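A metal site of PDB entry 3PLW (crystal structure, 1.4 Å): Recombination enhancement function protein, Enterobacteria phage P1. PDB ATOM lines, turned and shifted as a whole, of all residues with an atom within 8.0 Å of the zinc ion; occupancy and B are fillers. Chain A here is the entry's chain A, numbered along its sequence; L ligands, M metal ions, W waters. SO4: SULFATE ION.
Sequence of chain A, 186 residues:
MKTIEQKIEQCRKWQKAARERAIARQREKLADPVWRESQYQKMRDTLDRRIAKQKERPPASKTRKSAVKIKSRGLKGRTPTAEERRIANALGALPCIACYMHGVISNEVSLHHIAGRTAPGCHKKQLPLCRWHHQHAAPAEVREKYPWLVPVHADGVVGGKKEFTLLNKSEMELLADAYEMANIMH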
ATOM      1  N   SER A 110      -1.349 -28.101 -20.837  1.00  0.00           N
ATOM      2  CA  SER A 110      -2.016 -26.808 -20.681  1.00  0.00           C
ATOM      3  C   SER A 110      -2.212 -26.587 -19.191  1.00  0.00           C
ATOM      4  O   SER A 110      -2.136 -27.520 -18.393  1.00  0.00           O
ATOM      5  CB  SER A 110      -3.364 -26.776 -21.415  1.00  0.00           C
ATOM      6  OG  SER A 110      -4.255 -27.750 -20.931  1.00  0.00           O
ATOM      7  N   LEU A 111      -2.475 -25.339 -18.811  1.00  0.00           N
ATOM      8  CA  LEU A 111      -2.744 -25.025 -17.422  1.00  0.00           C
ATOM      9  C   LEU A 111      -4.217 -25.154 -17.070  1.00  0.00           C
ATOM     10  O   LEU A 111      -5.119 -24.717 -17.820  1.00  0.00           O
ATOM     11  CB  LEU A 111      -2.228 -23.641 -17.069  1.00  0.00           C
ATOM     12  CG  LEU A 111      -0.716 -23.444 -17.016  1.00  0.00           C
ATOM     13  CD1 LEU A 111      -0.392 -21.970 -16.777  1.00  0.00           C
ATOM     14  CD2 LEU A 111      -0.097 -24.270 -15.900  1.00  0.00           C
ATOM     15  N   HIS A 112      -4.447 -25.736 -15.899  1.00  0.00           N
ATOM     16  CA  HIS A 112      -5.771 -25.961 -15.338  1.00  0.00           C
ATOM     17  C   HIS A 112      -5.961 -25.117 -14.069  1.00  0.00           C
ATOM     18  O   HIS A 112      -5.172 -25.212 -13.129  1.00  0.00           O
ATOM     19  CB  HIS A 112      -5.920 -27.461 -15.012  1.00  0.00           C
ATOM     20  CG  HIS A 112      -7.043 -27.752 -14.062  1.00  0.00           C
ATOM     21  ND1 HIS A 112      -8.362 -27.637 -14.420  1.00  0.00           N
ATOM     22  CD2 HIS A 112      -7.036 -28.164 -12.770  1.00  0.00           C
ATOM     23  CE1 HIS A 112      -9.130 -27.968 -13.385  1.00  0.00           C
ATOM     24  NE2 HIS A 112      -8.346 -28.277 -12.381  1.00  0.00           N
ATOM     25  N   HIS A 113      -7.019 -24.307 -14.052  1.00  0.00           N
ATOM     26  CA  HIS A 113      -7.360 -23.531 -12.867  1.00  0.00           C
ATOM     27  C   HIS A 113      -8.028 -24.406 -11.831  1.00  0.00           C
ATOM     28  O   HIS A 113      -9.047 -25.045 -12.107  1.00  0.00           O
ATOM     29  CB  HIS A 113      -8.293 -22.368 -13.231  1.00  0.00           C
ATOM     30  CG  HIS A 113      -7.596 -21.217 -13.877  1.00  0.00           C
ATOM     31  ND1 HIS A 113      -7.491 -21.087 -15.236  1.00  0.00           N
ATOM     32  CD2 HIS A 113      -6.975 -20.143 -13.333  1.00  0.00           C
ATOM     33  CE1 HIS A 113      -6.831 -19.977 -15.521  1.00  0.00           C
ATOM     34  NE2 HIS A 113      -6.501 -19.389 -14.376  1.00  0.00           N
ATOM     35  N   ILE A 114      -7.467 -24.406 -10.626  1.00  0.00           N
ATOM     36  CA  ILE A 114      -8.001 -25.166  -9.500  1.00  0.00           C
ATOM     37  C   ILE A 114      -9.099 -24.397  -8.760  1.00  0.00           C
ATOM     38  O   ILE A 114     -10.069 -24.995  -8.283  1.00  0.00           O
ATOM     39  CB  ILE A 114      -6.901 -25.481  -8.466  1.00  0.00           C
ATOM     40  CG1 ILE A 114      -5.770 -26.309  -9.098  1.00  0.00           C
ATOM     41  CG2 ILE A 114      -7.483 -26.172  -7.235  1.00  0.00           C
ATOM     42  CD1 ILE A 114      -4.506 -26.279  -8.263  1.00  0.00           C
ATOM     43  N   ARG A 117     -11.125 -18.213 -11.774  1.00  0.00           N
ATOM     44  CA  ARG A 117     -10.376 -17.277 -12.586  1.00  0.00           C
ATOM     45  C   ARG A 117     -10.499 -15.831 -12.109  1.00  0.00           C
ATOM     46  O   ARG A 117     -10.038 -14.914 -12.794  1.00  0.00           O
ATOM     47  CB  ARG A 117     -10.813 -17.358 -14.050  1.00  0.00           C
ATOM     48  CG  ARG A 117     -10.414 -18.627 -14.764  1.00  0.00           C
ATOM     49  CD  ARG A 117     -11.115 -18.714 -16.117  1.00  0.00           C
ATOM     50  NE  ARG A 117     -10.519 -19.753 -16.953  1.00  0.00           N
ATOM     51  CZ  ARG A 117      -9.531 -19.540 -17.824  1.00  0.00           C
ATOM     52  NH1 ARG A 117      -9.006 -18.325 -17.979  1.00  0.00           N
ATOM     53  NH2 ARG A 117      -9.052 -20.544 -18.541  1.00  0.00           N
ATOM     54  N   GLN A 126      -2.721 -23.258 -10.348  1.00  0.00           N
ATOM     55  CA  GLN A 126      -2.974 -23.945 -11.612  1.00  0.00           C
ATOM     56  C   GLN A 126      -2.083 -25.168 -11.717  1.00  0.00           C
ATOM     57  O   GLN A 126      -0.950 -25.171 -11.226  1.00  0.00           O
ATOM     58  CB  GLN A 126      -2.714 -23.035 -12.815  1.00  0.00           C
ATOM     59  CG  GLN A 126      -3.510 -21.732 -12.779  1.00  0.00           C
ATOM     60  CD  GLN A 126      -3.431 -20.985 -14.072  1.00  0.00           C
ATOM     61  OE1 GLN A 126      -2.795 -19.913 -14.154  1.00  0.00           O
ATOM     62  NE2 GLN A 126      -4.050 -21.514 -15.102  1.00  0.00           N
ATOM     63  N   LEU A 127      -2.600 -26.204 -12.377  1.00  0.00           N
ATOM     64  CA  LEU A 127      -1.801 -27.411 -12.612  1.00  0.00           C
ATOM     65  C   LEU A 127      -1.470 -27.552 -14.089  1.00  0.00           C
ATOM     66  O   LEU A 127      -2.336 -27.380 -14.943  1.00  0.00           O
ATOM     67  CB  LEU A 127      -2.569 -28.662 -12.210  1.00  0.00           C
ATOM     68  CG  LEU A 127      -3.165 -28.737 -10.800  1.00  0.00           C
ATOM     69  CD1 LEU A 127      -3.938 -30.054 -10.621  1.00  0.00           C
ATOM     70  CD2 LEU A 127      -2.055 -28.633  -9.782  1.00  0.00           C
ATOM     71  N   LEU A 129      -1.292 -29.915 -16.964  1.00  0.00           N
ATOM     72  CA  LEU A 129      -1.907 -31.212 -17.231  1.00  0.00           C
ATOM     73  C   LEU A 129      -1.878 -31.539 -18.702  1.00  0.00           C
ATOM     74  O   LEU A 129      -2.080 -30.661 -19.537  1.00  0.00           O
ATOM     75  CB  LEU A 129      -3.361 -31.281 -16.714  1.00  0.00           C
ATOM     76  CG  LEU A 129      -3.586 -31.064 -15.222  1.00  0.00           C
ATOM     77  CD1 LEU A 129      -5.078 -30.992 -14.919  1.00  0.00           C
ATOM     78  CD2 LEU A 129      -2.925 -32.193 -14.401  1.00  0.00           C
ATOM     79  N   HIS A 133      -5.508 -35.644 -18.974  1.00  0.00           N
ATOM     80  CA  HIS A 133      -5.734 -35.318 -17.574  1.00  0.00           C
ATOM     81  C   HIS A 133      -6.481 -34.009 -17.421  1.00  0.00           C
ATOM     82  O   HIS A 133      -6.941 -33.689 -16.317  1.00  0.00           O
ATOM     83  CB  HIS A 133      -4.412 -35.227 -16.804  1.00  0.00           C
ATOM     84  CG  HIS A 133      -3.980 -36.513 -16.198  1.00  0.00           C
ATOM     85  ND1 HIS A 133      -2.718 -37.058 -16.411  1.00  0.00           N
ATOM     86  CD2 HIS A 133      -4.627 -37.362 -15.356  1.00  0.00           C
ATOM     87  CE1 HIS A 133      -2.620 -38.186 -15.729  1.00  0.00           C
ATOM     88  NE2 HIS A 133      -3.765 -38.385 -15.075  1.00  0.00           N
ATOM     89  N   HIS A 134      -6.628 -33.246 -18.515  1.00  0.00           N
ATOM     90  CA  HIS A 134      -7.344 -31.979 -18.418  1.00  0.00           C
ATOM     91  C   HIS A 134      -8.798 -32.059 -18.881  1.00  0.00           C
ATOM     92  O   HIS A 134      -9.706 -31.964 -18.051  1.00  0.00           O
ATOM     93  CB  HIS A 134      -6.602 -30.830 -19.109  1.00  0.00           C
ATOM     94  CG  HIS A 134      -7.080 -29.486 -18.650  1.00  0.00           C
ATOM     95  ND1 HIS A 134      -6.858 -28.321 -19.364  1.00  0.00           N
ATOM     96  CD2 HIS A 134      -7.811 -29.124 -17.567  1.00  0.00           C
ATOM     97  CE1 HIS A 134      -7.409 -27.300 -18.721  1.00  0.00           C
ATOM     98  NE2 HIS A 134      -7.995 -27.762 -17.633  1.00  0.00           N
ATOM     99  N   GLN A 135      -9.019 -32.249 -20.181  1.00  0.00           N
ATOM    100  CA  GLN A 135     -10.387 -32.187 -20.724  1.00  0.00           C
ATOM    101  C   GLN A 135     -10.815 -33.376 -21.579  1.00  0.00           C
ATOM    102  O   GLN A 135     -12.004 -33.506 -21.872  1.00  0.00           O
ATOM    103  CB  GLN A 135     -10.602 -30.899 -21.530  1.00  0.00           C
ATOM    104  CG  GLN A 135     -10.439 -29.613 -20.763  1.00  0.00           C
ATOM    105  CD  GLN A 135     -10.682 -28.408 -21.632  1.00  0.00           C
ATOM    106  OE1 GLN A 135      -9.739 -27.779 -22.131  1.00  0.00           O
ATOM    107  NE2 GLN A 135     -11.947 -28.069 -21.831  1.00  0.00           N
ATOM    108  N   VAL A 152      -9.676 -34.068 -15.393  1.00  0.00           N
ATOM    109  CA  VAL A 152     -10.207 -33.389 -14.217  1.00  0.00           C
ATOM    110  C   VAL A 152     -11.534 -32.681 -14.530  1.00  0.00           C
ATOM    111  O   VAL A 152     -12.379 -32.541 -13.636  1.00  0.00           O
ATOM    112  CB  VAL A 152      -9.162 -32.435 -13.616  1.00  0.00           C
ATOM    113  CG1 VAL A 152      -8.910 -31.227 -14.526  1.00  0.00           C
ATOM    114  CG2 VAL A 152      -9.565 -31.963 -12.207  1.00  0.00           C
ATOM    115  N   HIS A 153     -11.726 -32.272 -15.781  1.00  0.00           N
ATOM    116  CA  HIS A 153     -13.054 -31.885 -16.285  1.00  0.00           C
ATOM    117  C   HIS A 153     -13.663 -33.104 -16.962  1.00  0.00           C
ATOM    118  O   HIS A 153     -13.106 -33.606 -17.939  1.00  0.00           O
ATOM    119  CB  HIS A 153     -12.965 -30.742 -17.315  1.00  0.00           C
ATOM    120  CG  HIS A 153     -12.309 -29.506 -16.791  1.00  0.00           C
ATOM    121  ND1 HIS A 153     -12.918 -28.651 -15.899  1.00  0.00           N
ATOM    122  CD2 HIS A 153     -11.092 -28.976 -17.053  1.00  0.00           C
ATOM    123  CE1 HIS A 153     -12.090 -27.650 -15.627  1.00  0.00           C
ATOM    124  NE2 HIS A 153     -10.975 -27.826 -16.316  1.00  0.00           N
ATOM    125  N   GLU A 171      -6.160 -31.800  -6.079  1.00  0.00           N
ATOM    126  CA  GLU A 171      -5.575 -30.722  -6.861  1.00  0.00           C
ATOM    127  C   GLU A 171      -4.550 -29.895  -6.072  1.00  0.00           C
ATOM    128  O   GLU A 171      -3.493 -29.579  -6.606  1.00  0.00           O
ATOM    129  CB  GLU A 171      -6.652 -29.808  -7.447  1.00  0.00           C
ATOM    130  CG  GLU A 171      -7.552 -30.479  -8.504  1.00  0.00           C
ATOM    131  CD  GLU A 171      -8.793 -29.648  -8.760  1.00  0.00           C
ATOM    132  OE1 GLU A 171      -8.920 -29.065  -9.850  1.00  0.00           O
ATOM    133  OE2 GLU A 171      -9.630 -29.547  -7.836  1.00  0.00           O
HETATM  134  S   SO4 L   1      -9.573 -23.974 -16.983  1.00  0.00           S
HETATM  135  O1  SO4 L   1      -9.796 -24.426 -18.350  1.00  0.00           O
HETATM  136  O2  SO4 L   1     -10.856 -23.705 -16.324  1.00  0.00           O
HETATM  137  O3  SO4 L   1      -8.783 -22.743 -16.959  1.00  0.00           O
HETATM  138  O4  SO4 L   1      -8.855 -25.020 -16.207  1.00  0.00           O
HETATM  139 ZN    ZN M   1      -9.175 -26.909 -16.197  1.00  0.00          ZN
HETATM  140  O   HOH W   1     -11.018 -25.112 -14.049  1.00  0.00           O
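The backbone carbonyl oxygen (O) of His 134 lies within hydrogen-bond range of the backbone NH (N) of Val 152 (3.4 Å). ND1 of His 134 lies within hydrogen-bond range of OG of Ser 110, 3.1 Å away. OE1 of Glu 171 lies within hydrogen-bond range of NE2 of His 112, at 2.7 Å. The backbone carbonyl oxygen (O) of Leu 127 sits at hydrogen-bond distance from the backbone NH (N) of His 112 (2.8 Å).
Of the 15 residues printed, 3 come within 4 Å of the zinc ion. The nearest printed residue that does not touch the zinc ion is His 113 (4.002 Å).
The zinc ion is bound by an oxygen (O4) of the ligand (1.9 Å), a ring nitrogen (NE2) of His 153 (2.0 Å), a ring nitrogen (NE2) of His 134 (2.0 Å) and a ring nitrogen (ND1) of His 112 (2.1 Å). The zinc ion has four donor atoms within binding distance.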
